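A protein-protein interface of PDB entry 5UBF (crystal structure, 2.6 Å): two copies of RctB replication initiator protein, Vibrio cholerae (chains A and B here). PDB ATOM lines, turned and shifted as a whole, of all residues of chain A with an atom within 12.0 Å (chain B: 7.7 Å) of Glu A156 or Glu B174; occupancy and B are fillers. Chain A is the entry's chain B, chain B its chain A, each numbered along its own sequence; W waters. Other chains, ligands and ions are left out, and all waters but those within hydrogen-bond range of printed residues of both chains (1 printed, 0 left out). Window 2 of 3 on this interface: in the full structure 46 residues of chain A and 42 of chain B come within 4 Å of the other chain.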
ATOM      1  N   THR A  55     -24.169   1.970   1.555  1.00  0.00           N
ATOM      2  CA  THR A  55     -23.014   2.859   1.556  1.00  0.00           C
ATOM      3  C   THR A  55     -21.741   2.051   1.330  1.00  0.00           C
ATOM      4  O   THR A  55     -21.426   1.146   2.111  1.00  0.00           O
ATOM      5  CB  THR A  55     -22.932   3.627   2.873  1.00  0.00           C
ATOM      6  OG1 THR A  55     -24.094   4.455   3.018  1.00  0.00           O
ATOM      7  CG2 THR A  55     -21.683   4.498   2.905  1.00  0.00           C
ATOM      8  N   ARG A  56     -21.016   2.377   0.265  1.00  0.00           N
ATOM      9  CA  ARG A  56     -19.731   1.749  -0.005  1.00  0.00           C
ATOM     10  C   ARG A  56     -18.643   2.396   0.842  1.00  0.00           C
ATOM     11  O   ARG A  56     -18.595   3.621   0.990  1.00  0.00           O
ATOM     12  CB  ARG A  56     -19.382   1.867  -1.489  1.00  0.00           C
ATOM     13  CG  ARG A  56     -19.651   3.248  -2.063  1.00  0.00           C
ATOM     14  CD  ARG A  56     -18.770   3.543  -3.262  1.00  0.00           C
ATOM     15  NE  ARG A  56     -18.933   4.922  -3.714  1.00  0.00           N
ATOM     16  CZ  ARG A  56     -18.116   5.531  -4.565  1.00  0.00           C
ATOM     17  NH1 ARG A  56     -17.067   4.888  -5.060  1.00  0.00           N
ATOM     18  NH2 ARG A  56     -18.344   6.789  -4.919  1.00  0.00           N
ATOM     19  N   HIS A 143     -13.561   3.852   6.243  1.00  0.00           N
ATOM     20  CA  HIS A 143     -13.700   5.153   5.602  1.00  0.00           C
ATOM     21  C   HIS A 143     -14.918   5.123   4.688  1.00  0.00           C
ATOM     22  O   HIS A 143     -14.947   4.362   3.714  1.00  0.00           O
ATOM     23  CB  HIS A 143     -12.448   5.509   4.799  1.00  0.00           C
ATOM     24  CG  HIS A 143     -11.168   5.333   5.555  1.00  0.00           C
ATOM     25  ND1 HIS A 143     -10.534   6.374   6.198  1.00  0.00           N
ATOM     26  CD2 HIS A 143     -10.400   4.238   5.762  1.00  0.00           C
ATOM     27  CE1 HIS A 143      -9.432   5.927   6.772  1.00  0.00           C
ATOM     28  NE2 HIS A 143      -9.327   4.634   6.524  1.00  0.00           N
ATOM     29  N   GLU A 144     -15.915   5.949   4.996  1.00  0.00           N
ATOM     30  CA  GLU A 144     -17.105   6.046   4.161  1.00  0.00           C
ATOM     31  C   GLU A 144     -16.839   6.976   2.985  1.00  0.00           C
ATOM     32  O   GLU A 144     -16.322   8.083   3.161  1.00  0.00           O
ATOM     33  CB  GLU A 144     -18.294   6.546   4.978  1.00  0.00           C
ATOM     34  CG  GLU A 144     -18.750   5.583   6.060  1.00  0.00           C
ATOM     35  CD  GLU A 144     -19.971   6.084   6.806  1.00  0.00           C
ATOM     36  OE1 GLU A 144     -20.455   7.188   6.481  1.00  0.00           O
ATOM     37  OE2 GLU A 144     -20.447   5.373   7.717  1.00  0.00           O
ATOM     38  N   LEU A 145     -17.196   6.525   1.784  1.00  0.00           N
ATOM     39  CA  LEU A 145     -16.924   7.279   0.568  1.00  0.00           C
ATOM     40  C   LEU A 145     -18.049   8.230   0.183  1.00  0.00           C
ATOM     41  O   LEU A 145     -17.854   9.064  -0.708  1.00  0.00           O
ATOM     42  CB  LEU A 145     -16.648   6.320  -0.596  1.00  0.00           C
ATOM     43  CG  LEU A 145     -15.471   5.357  -0.423  1.00  0.00           C
ATOM     44  CD1 LEU A 145     -15.264   4.535  -1.684  1.00  0.00           C
ATOM     45  CD2 LEU A 145     -14.201   6.110  -0.057  1.00  0.00           C
ATOM     46  N   THR A 146     -19.212   8.130   0.822  1.00  0.00           N
ATOM     47  CA  THR A 146     -20.351   8.985   0.516  1.00  0.00           C
ATOM     48  C   THR A 146     -20.478  10.053   1.597  1.00  0.00           C
ATOM     49  O   THR A 146     -20.593   9.729   2.784  1.00  0.00           O
ATOM     50  CB  THR A 146     -21.639   8.167   0.415  1.00  0.00           C
ATOM     51  OG1 THR A 146     -21.912   7.546   1.677  1.00  0.00           O
ATOM     52  CG2 THR A 146     -21.503   7.092  -0.655  1.00  0.00           C
ATOM     53  N   GLY A 147     -20.455  11.316   1.183  1.00  0.00           N
ATOM     54  CA  GLY A 147     -20.558  12.403   2.140  1.00  0.00           C
ATOM     55  C   GLY A 147     -21.950  12.489   2.742  1.00  0.00           C
ATOM     56  O   GLY A 147     -22.958  12.253   2.075  1.00  0.00           O
ATOM     57  N   ARG A 148     -21.997  12.830   4.026  1.00  0.00           N
ATOM     58  CA  ARG A 148     -23.241  12.973   4.764  1.00  0.00           C
ATOM     59  C   ARG A 148     -23.313  14.362   5.383  1.00  0.00           C
ATOM     60  O   ARG A 148     -22.297  15.042   5.559  1.00  0.00           O
ATOM     61  CB  ARG A 148     -23.366  11.915   5.869  1.00  0.00           C
ATOM     62  CG  ARG A 148     -23.184  10.478   5.409  1.00  0.00           C
ATOM     63  CD  ARG A 148     -24.413   9.956   4.685  1.00  0.00           C
ATOM     64  NE  ARG A 148     -24.726   8.585   5.081  1.00  0.00           N
ATOM     65  CZ  ARG A 148     -24.151   7.504   4.564  1.00  0.00           C
ATOM     66  NH1 ARG A 148     -23.223   7.629   3.625  1.00  0.00           N
ATOM     67  NH2 ARG A 148     -24.500   6.297   4.989  1.00  0.00           N
ATOM     68  N   TRP A 149     -24.530  14.779   5.716  1.00  0.00           N
ATOM     69  CA  TRP A 149     -24.727  16.020   6.449  1.00  0.00           C
ATOM     70  C   TRP A 149     -24.562  15.760   7.939  1.00  0.00           C
ATOM     71  O   TRP A 149     -25.138  14.809   8.479  1.00  0.00           O
ATOM     72  CB  TRP A 149     -26.109  16.603   6.159  1.00  0.00           C
ATOM     73  CG  TRP A 149     -26.394  17.878   6.898  1.00  0.00           C
ATOM     74  CD1 TRP A 149     -26.179  19.150   6.450  1.00  0.00           C
ATOM     75  CD2 TRP A 149     -26.948  18.004   8.213  1.00  0.00           C
ATOM     76  NE1 TRP A 149     -26.566  20.059   7.406  1.00  0.00           N
ATOM     77  CE2 TRP A 149     -27.041  19.380   8.498  1.00  0.00           C
ATOM     78  CE3 TRP A 149     -27.375  17.085   9.177  1.00  0.00           C
ATOM     79  CZ2 TRP A 149     -27.543  19.861   9.706  1.00  0.00           C
ATOM     80  CZ3 TRP A 149     -27.873  17.564  10.375  1.00  0.00           C
ATOM     81  CH2 TRP A 149     -27.952  18.939  10.628  1.00  0.00           C
ATOM     82  N   LEU A 150     -23.773  16.602   8.603  1.00  0.00           N
ATOM     83  CA  LEU A 150     -23.487  16.432  10.021  1.00  0.00           C
ATOM     84  C   LEU A 150     -24.029  17.570  10.869  1.00  0.00           C
ATOM     85  O   LEU A 150     -24.692  17.320  11.884  1.00  0.00           O
ATOM     86  CB  LEU A 150     -21.972  16.289  10.233  1.00  0.00           C
ATOM     87  CG  LEU A 150     -21.326  15.113   9.498  1.00  0.00           C
ATOM     88  CD1 LEU A 150     -19.825  15.111   9.710  1.00  0.00           C
ATOM     89  CD2 LEU A 150     -21.939  13.796   9.950  1.00  0.00           C
ATOM     90  N   SER A 151     -23.771  18.816  10.486  1.00  0.00           N
ATOM     91  CA  SER A 151     -24.242  19.967  11.243  1.00  0.00           C
ATOM     92  C   SER A 151     -24.315  21.162  10.302  1.00  0.00           C
ATOM     93  O   SER A 151     -24.019  21.058   9.108  1.00  0.00           O
ATOM     94  CB  SER A 151     -23.332  20.250  12.442  1.00  0.00           C
ATOM     95  OG  SER A 151     -22.013  20.548  12.018  1.00  0.00           O
ATOM     96  N   GLU A 152     -24.719  22.308  10.856  1.00  0.00           N
ATOM     97  CA  GLU A 152     -24.768  23.533  10.066  1.00  0.00           C
ATOM     98  C   GLU A 152     -23.377  23.962   9.616  1.00  0.00           C
ATOM     99  O   GLU A 152     -23.225  24.523   8.524  1.00  0.00           O
ATOM    100  CB  GLU A 152     -25.434  24.651  10.868  1.00  0.00           C
ATOM    101  CG  GLU A 152     -26.818  24.303  11.394  1.00  0.00           C
ATOM    102  CD  GLU A 152     -27.401  25.399  12.265  1.00  0.00           C
ATOM    103  OE1 GLU A 152     -26.749  26.454  12.413  1.00  0.00           O
ATOM    104  OE2 GLU A 152     -28.512  25.206  12.804  1.00  0.00           O
ATOM    105  N   ASN A 153     -22.355  23.704  10.436  1.00  0.00           N
ATOM    106  CA  ASN A 153     -20.995  24.093  10.081  1.00  0.00           C
ATOM    107  C   ASN A 153     -20.350  23.109   9.112  1.00  0.00           C
ATOM    108  O   ASN A 153     -19.469  23.499   8.339  1.00  0.00           O
ATOM    109  CB  ASN A 153     -20.142  24.229  11.344  1.00  0.00           C
ATOM    110  CG  ASN A 153     -20.654  25.307  12.280  1.00  0.00           C
ATOM    111  OD1 ASN A 153     -21.316  26.254  11.853  1.00  0.00           O
ATOM    112  ND2 ASN A 153     -20.347  25.169  13.564  1.00  0.00           N
ATOM    113  N   MET A 154     -20.763  21.844   9.140  1.00  0.00           N
ATOM    114  CA  MET A 154     -20.276  20.862   8.174  1.00  0.00           C
ATOM    115  C   MET A 154     -21.410  20.344   7.296  1.00  0.00           C
ATOM    116  O   MET A 154     -22.089  19.380   7.654  1.00  0.00           O
ATOM    117  CB  MET A 154     -19.585  19.690   8.878  1.00  0.00           C
ATOM    118  CG  MET A 154     -18.195  20.013   9.400  1.00  0.00           C
ATOM    119  SD  MET A 154     -17.105  18.425   9.676  1.00  0.00           S
ATOM    120  CE  MET A 154     -16.867  17.897   7.797  1.00  0.00           C
ATOM    121  N   PRO A 155     -21.614  20.985   6.142  1.00  0.00           N
ATOM    122  CA  PRO A 155     -22.676  20.514   5.237  1.00  0.00           C
ATOM    123  C   PRO A 155     -22.386  19.149   4.642  1.00  0.00           C
ATOM    124  O   PRO A 155     -23.290  18.307   4.568  1.00  0.00           O
ATOM    125  CB  PRO A 155     -22.730  21.610   4.164  1.00  0.00           C
ATOM    126  CG  PRO A 155     -21.364  22.218   4.183  1.00  0.00           C
ATOM    127  CD  PRO A 155     -20.921  22.174   5.616  1.00  0.00           C
ATOM    128  N   GLU A 156     -21.151  18.904   4.214  1.00  0.00           N
ATOM    129  CA  GLU A 156     -20.740  17.617   3.668  1.00  0.00           C
ATOM    130  C   GLU A 156     -19.625  17.063   4.540  1.00  0.00           C
ATOM    131  O   GLU A 156     -18.586  17.710   4.710  1.00  0.00           O
ATOM    132  CB  GLU A 156     -20.275  17.753   2.216  1.00  0.00           C
ATOM    133  CG  GLU A 156     -19.969  16.426   1.542  1.00  0.00           C
ATOM    134  CD  GLU A 156     -19.361  16.597   0.163  1.00  0.00           C
ATOM    135  OE1 GLU A 156     -18.737  17.649  -0.088  1.00  0.00           O
ATOM    136  OE2 GLU A 156     -19.508  15.677  -0.670  1.00  0.00           O
ATOM    137  N   GLY A 157     -19.843  15.873   5.095  1.00  0.00           N
ATOM    138  CA  GLY A 157     -18.867  15.278   5.985  1.00  0.00           C
ATOM    139  C   GLY A 157     -18.627  13.805   5.734  1.00  0.00           C
ATOM    140  O   GLY A 157     -19.564  13.002   5.743  1.00  0.00           O
ATOM    141  N   PHE A 158     -17.369  13.441   5.503  1.00  0.00           N
ATOM    142  CA  PHE A 158     -16.982  12.047   5.336  1.00  0.00           C
ATOM    143  C   PHE A 158     -16.520  11.490   6.676  1.00  0.00           C
ATOM    144  O   PHE A 158     -15.672  12.089   7.346  1.00  0.00           O
ATOM    145  CB  PHE A 158     -15.875  11.914   4.290  1.00  0.00           C
ATOM    146  CG  PHE A 158     -16.288  12.346   2.913  1.00  0.00           C
ATOM    147  CD1 PHE A 158     -16.208  13.676   2.536  1.00  0.00           C
ATOM    148  CD2 PHE A 158     -16.757  11.422   1.995  1.00  0.00           C
ATOM    149  CE1 PHE A 158     -16.587  14.076   1.271  1.00  0.00           C
ATOM    150  CE2 PHE A 158     -17.137  11.816   0.727  1.00  0.00           C
ATOM    151  CZ  PHE A 158     -17.052  13.146   0.364  1.00  0.00           C
ATOM    152  N   LYS A 159     -17.082  10.351   7.064  1.00  0.00           N
ATOM    153  CA  LYS A 159     -16.832   9.756   8.370  1.00  0.00           C
ATOM    154  C   LYS A 159     -15.829   8.616   8.250  1.00  0.00           C
ATOM    155  O   LYS A 159     -15.971   7.744   7.388  1.00  0.00           O
ATOM    156  CB  LYS A 159     -18.135   9.244   8.986  1.00  0.00           C
ATOM    157  CG  LYS A 159     -17.950   8.494  10.296  1.00  0.00           C
ATOM    158  CD  LYS A 159     -19.244   7.834  10.742  1.00  0.00           C
ATOM    159  CE  LYS A 159     -19.038   7.005  11.999  1.00  0.00           C
ATOM    160  NZ  LYS A 159     -20.272   6.270  12.392  1.00  0.00           N
ATOM    161  N   SER A 160     -14.818   8.632   9.116  1.00  0.00           N
ATOM    162  CA  SER A 160     -13.876   7.534   9.264  1.00  0.00           C
ATOM    163  C   SER A 160     -13.864   7.085  10.718  1.00  0.00           C
ATOM    164  O   SER A 160     -13.972   7.910  11.631  1.00  0.00           O
ATOM    165  CB  SER A 160     -12.463   7.934   8.827  1.00  0.00           C
ATOM    166  OG  SER A 160     -12.381   8.079   7.422  1.00  0.00           O
ATOM    167  N   ARG B 125      -2.855  22.784   9.324  1.00  0.00           N
ATOM    168  CA  ARG B 125      -3.790  21.682   9.525  1.00  0.00           C
ATOM    169  C   ARG B 125      -3.131  20.340   9.232  1.00  0.00           C
ATOM    170  O   ARG B 125      -3.357  19.362   9.952  1.00  0.00           O
ATOM    171  CB  ARG B 125      -5.028  21.873   8.649  1.00  0.00           C
ATOM    172  CG  ARG B 125      -5.960  22.982   9.112  1.00  0.00           C
ATOM    173  CD  ARG B 125      -7.050  23.248   8.083  1.00  0.00           C
ATOM    174  NE  ARG B 125      -7.931  24.340   8.485  1.00  0.00           N
ATOM    175  CZ  ARG B 125      -9.130  24.172   9.033  1.00  0.00           C
ATOM    176  NH1 ARG B 125      -9.601  22.950   9.242  1.00  0.00           N
ATOM    177  NH2 ARG B 125      -9.861  25.225   9.369  1.00  0.00           N
ATOM    178  N   ARG B 129      -2.651  17.430  12.001  1.00  0.00           N
ATOM    179  CA  ARG B 129      -3.180  16.109  11.679  1.00  0.00           C
ATOM    180  C   ARG B 129      -2.093  15.046  11.714  1.00  0.00           C
ATOM    181  O   ARG B 129      -2.368  13.891  12.058  1.00  0.00           O
ATOM    182  CB  ARG B 129      -3.856  16.125  10.305  1.00  0.00           C
ATOM    183  CG  ARG B 129      -5.160  16.904  10.247  1.00  0.00           C
ATOM    184  CD  ARG B 129      -5.813  16.762   8.881  1.00  0.00           C
ATOM    185  NE  ARG B 129      -6.972  17.635   8.726  1.00  0.00           N
ATOM    186  CZ  ARG B 129      -7.027  18.662   7.885  1.00  0.00           C
ATOM    187  NH1 ARG B 129      -5.989  18.942   7.108  1.00  0.00           N
ATOM    188  NH2 ARG B 129      -8.125  19.402   7.811  1.00  0.00           N
ATOM    189  N   THR B 171     -13.696  10.249  13.112  1.00  0.00           N
ATOM    190  CA  THR B 171     -13.280  11.498  12.492  1.00  0.00           C
ATOM    191  C   THR B 171     -14.300  11.949  11.460  1.00  0.00           C
ATOM    192  O   THR B 171     -14.926  11.134  10.778  1.00  0.00           O
ATOM    193  CB  THR B 171     -11.898  11.371  11.832  1.00  0.00           C
ATOM    194  OG1 THR B 171     -11.853  10.184  11.031  1.00  0.00           O
ATOM    195  CG2 THR B 171     -10.802  11.315  12.888  1.00  0.00           C
ATOM    196  N   ALA B 172     -14.458  13.267  11.356  1.00  0.00           N
ATOM    197  CA  ALA B 172     -15.328  13.889  10.367  1.00  0.00           C
ATOM    198  C   ALA B 172     -14.484  14.797   9.486  1.00  0.00           C
ATOM    199  O   ALA B 172     -13.890  15.766   9.976  1.00  0.00           O
ATOM    200  CB  ALA B 172     -16.456  14.676  11.035  1.00  0.00           C
ATOM    201  N   SER B 173     -14.430  14.476   8.196  1.00  0.00           N
ATOM    202  CA  SER B 173     -13.628  15.195   7.219  1.00  0.00           C
ATOM    203  C   SER B 173     -14.530  15.906   6.219  1.00  0.00           C
ATOM    204  O   SER B 173     -15.611  15.419   5.877  1.00  0.00           O
ATOM    205  CB  SER B 173     -12.691  14.243   6.468  1.00  0.00           C
ATOM    206  OG  SER B 173     -12.128  13.278   7.339  1.00  0.00           O
ATOM    207  N   GLU B 174     -14.072  17.065   5.747  1.00  0.00           N
ATOM    208  CA  GLU B 174     -14.812  17.806   4.733  1.00  0.00           C
ATOM    209  C   GLU B 174     -14.448  17.364   3.321  1.00  0.00           C
ATOM    210  O   GLU B 174     -15.335  17.208   2.474  1.00  0.00           O
ATOM    211  CB  GLU B 174     -14.570  19.309   4.890  1.00  0.00           C
ATOM    212  CG  GLU B 174     -15.403  20.165   3.951  1.00  0.00           C
ATOM    213  CD  GLU B 174     -15.263  21.648   4.234  1.00  0.00           C
ATOM    214  OE1 GLU B 174     -14.480  22.009   5.136  1.00  0.00           O
ATOM    215  OE2 GLU B 174     -15.939  22.450   3.557  1.00  0.00           O
ATOM    216  N   GLU B 175     -13.163  17.157   3.049  1.00  0.00           N
ATOM    217  CA  GLU B 175     -12.745  16.640   1.757  1.00  0.00           C
ATOM    218  C   GLU B 175     -12.976  15.133   1.687  1.00  0.00           C
ATOM    219  O   GLU B 175     -13.172  14.458   2.702  1.00  0.00           O
ATOM    220  CB  GLU B 175     -11.271  16.955   1.492  1.00  0.00           C
ATOM    221  CG  GLU B 175     -10.965  18.426   1.248  1.00  0.00           C
ATOM    222  CD  GLU B 175     -10.892  19.237   2.528  1.00  0.00           C
ATOM    223  OE1 GLU B 175     -11.040  18.650   3.621  1.00  0.00           O
ATOM    224  OE2 GLU B 175     -10.681  20.467   2.441  1.00  0.00           O
ATOM    225  N   ALA B 176     -12.950  14.610   0.467  1.00  0.00           N
ATOM    226  CA  ALA B 176     -13.178  13.193   0.246  1.00  0.00           C
ATOM    227  C   ALA B 176     -11.925  12.383   0.580  1.00  0.00           C
ATOM    228  O   ALA B 176     -10.807  12.904   0.523  1.00  0.00           O
ATOM    229  CB  ALA B 176     -13.585  12.941  -1.202  1.00  0.00           C
ATOM    230  N   PRO B 177     -12.089  11.112   0.948  1.00  0.00           N
ATOM    231  CA  PRO B 177     -10.918  10.251   1.160  1.00  0.00           C
ATOM    232  C   PRO B 177     -10.105  10.112  -0.120  1.00  0.00           C
ATOM    233  O   PRO B 177     -10.640   9.804  -1.188  1.00  0.00           O
ATOM    234  CB  PRO B 177     -11.534   8.914   1.588  1.00  0.00           C
ATOM    235  CG  PRO B 177     -12.871   9.274   2.143  1.00  0.00           C
ATOM    236  CD  PRO B 177     -13.344  10.442   1.328  1.00  0.00           C
ATOM    237  N   LYS B 188      -8.443  13.872   5.628  1.00  0.00           N
ATOM    238  CA  LYS B 188      -8.200  15.221   6.138  1.00  0.00           C
ATOM    239  C   LYS B 188      -9.322  15.582   7.101  1.00  0.00           C
ATOM    240  O   LYS B 188     -10.207  16.383   6.776  1.00  0.00           O
ATOM    241  CB  LYS B 188      -8.107  16.235   4.997  1.00  0.00           C
ATOM    242  CG  LYS B 188      -6.970  15.980   4.026  1.00  0.00           C
ATOM    243  CD  LYS B 188      -6.997  16.977   2.880  1.00  0.00           C
ATOM    244  CE  LYS B 188      -6.906  18.405   3.390  1.00  0.00           C
ATOM    245  NZ  LYS B 188      -6.941  19.392   2.278  1.00  0.00           N
ATOM    246  N   PRO B 189      -9.316  15.006   8.301  1.00  0.00           N
ATOM    247  CA  PRO B 189     -10.432  15.220   9.224  1.00  0.00           C
ATOM    248  C   PRO B 189     -10.470  16.644   9.754  1.00  0.00           C
ATOM    249  O   PRO B 189      -9.481  17.378   9.738  1.00  0.00           O
ATOM    250  CB  PRO B 189     -10.157  14.220  10.352  1.00  0.00           C
ATOM    251  CG  PRO B 189      -8.685  14.020  10.318  1.00  0.00           C
ATOM    252  CD  PRO B 189      -8.286  14.121   8.873  1.00  0.00           C
ATOM    253  N   ASN B 190     -11.657  17.033  10.211  1.00  0.00           N
ATOM    254  CA  ASN B 190     -11.843  18.283  10.934  1.00  0.00           C
ATOM    255  C   ASN B 190     -12.476  18.107  12.303  1.00  0.00           C
ATOM    256  O   ASN B 190     -12.328  19.001  13.144  1.00  0.00           O
ATOM    257  CB  ASN B 190     -12.695  19.266  10.116  1.00  0.00           C
ATOM    258  CG  ASN B 190     -11.983  19.754   8.870  1.00  0.00           C
ATOM    259  OD1 ASN B 190     -11.100  20.609   8.942  1.00  0.00           O
ATOM    260  ND2 ASN B 190     -12.372  19.219   7.718  1.00  0.00           N
ATOM    261  N   LEU B 191     -13.166  16.999  12.561  1.00  0.00           N
ATOM    262  CA  LEU B 191     -13.733  16.718  13.873  1.00  0.00           C
ATOM    263  C   LEU B 191     -13.155  15.415  14.404  1.00  0.00           C
ATOM    264  O   LEU B 191     -13.133  14.403  13.692  1.00  0.00           O
ATOM    265  CB  LEU B 191     -15.260  16.643  13.814  1.00  0.00           C
ATOM    266  CG  LEU B 191     -15.977  16.353  15.134  1.00  0.00           C
ATOM    267  CD1 LEU B 191     -15.525  17.321  16.214  1.00  0.00           C
ATOM    268  CD2 LEU B 191     -17.484  16.422  14.951  1.00  0.00           C
HETATM  269  O   HOH W   1     -12.544  11.008   5.872  1.00  0.00           O
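Glu A144 touches Pro B177. CD1 of Leu A150 touches CB of Ala B172, at 3.6 Å. Met A154 touches Ser B173. CE of Met A154 touches N of Glu B174, at 3.6 Å. Ser B173 touches Glu A156. Phe A158 touches Thr B171. O of Glu B174 touches CE1 of Phe A158, at 3.6 Å. Phe A158 touches Glu B175 (CD1 to O, 3.1 Å). Phe A158 touches Ala B176. Thr B171 touches Lys A159 (O to CA, 3.4 Å).
No position is printed for both chains. Of the 16 pairs that touch across the chains among the printed residues, none has its exchanged pair printed and touching as well.
Of the 20 printed residues of chain A, 8 touch a printed residue of chain B. Hydrophobic or aromatic side chains of chain A within 4 Å of the printed part of chain B: Leu A150, Met A154 and Phe A158. Among the printed residues, 16 pairs touch across the chains.
Of the printed residues of chain B, Glu A144 touches Pro B177. Printed residues of chain B within 4 Å of Met A154: Ser B173 (3.4 Å) and Glu B174 (3.6 Å). No residue of chain B comes within 4 Å of Pro A155. Of chain B, only Ser B173 (3.9 Å) and Glu B174 (3.8 Å) come within 4 Å of Glu A156. Printed residues of chain B within 4 Å of Ser A160: Thr B171 (2.8 Å). Of the printed residues of chain A, Thr B171 touches Phe A158, Lys A159 and Ser A160. Of chain A, only Leu A150 (3.6 Å) and Phe A158 (3.5 Å) come within 4 Å of Ala B172. Ser B173 touches four residues of chain A. Glu B174 touches just these residues of chain A: Met A154, Glu A156 and Phe A158. Glu B175 touches just one residue of chain A: Phe A158. Pro B189 touches none of the printed residues of chain A. No residue of chain A comes within 4 Å of Asn B190. The nearest residue of chain B that does not touch Glu A156 is Glu B175 (5.7 Å). The nearest residue of chain A that does not touch Glu B174 is Gly A157 (4.9 Å). The nearest printed residue of chain B that does not touch Ser A160 is Ala B172 (5.2 Å).
Water W1 lies within hydrogen-bond range of the side-chain hydroxyl (OG) of Ser B173 (2.7 Å) and the side-chain hydroxyl (OG) of Ser A160 (3.3 Å).
N of Phe A158 lies within hydrogen-bond range of O of Ser B173 (2.7 Å). The backbone NH of Thr B171 lies within hydrogen-bond range of the backbone carbonyl oxygen of Ser A160.
The backbone NH (N) of Glu B174 lies close to the side-chain amide nitrogen (ND2) of Asn B190. OG of Ser A160 is in hydrogen-bond range of ND1 of His A143 (2.8 Å). The side-chain amino group (NZ) of Lys B188 is in salt-bridge range of the side-chain carboxylate (OE2) of Glu B175 (3.9 Å). The backbone NH of Ala B172 sits at hydrogen-bond distance from the backbone carbonyl oxygen of Leu B191 (2.9 Å). The backbone carbonyl oxygen of Ala B172 sits at hydrogen-bond distance from the backbone NH of Asn B190, at 2.6 Å. O of Lys A159 sits at hydrogen-bond distance from N of Glu A144, at 3.0 Å.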
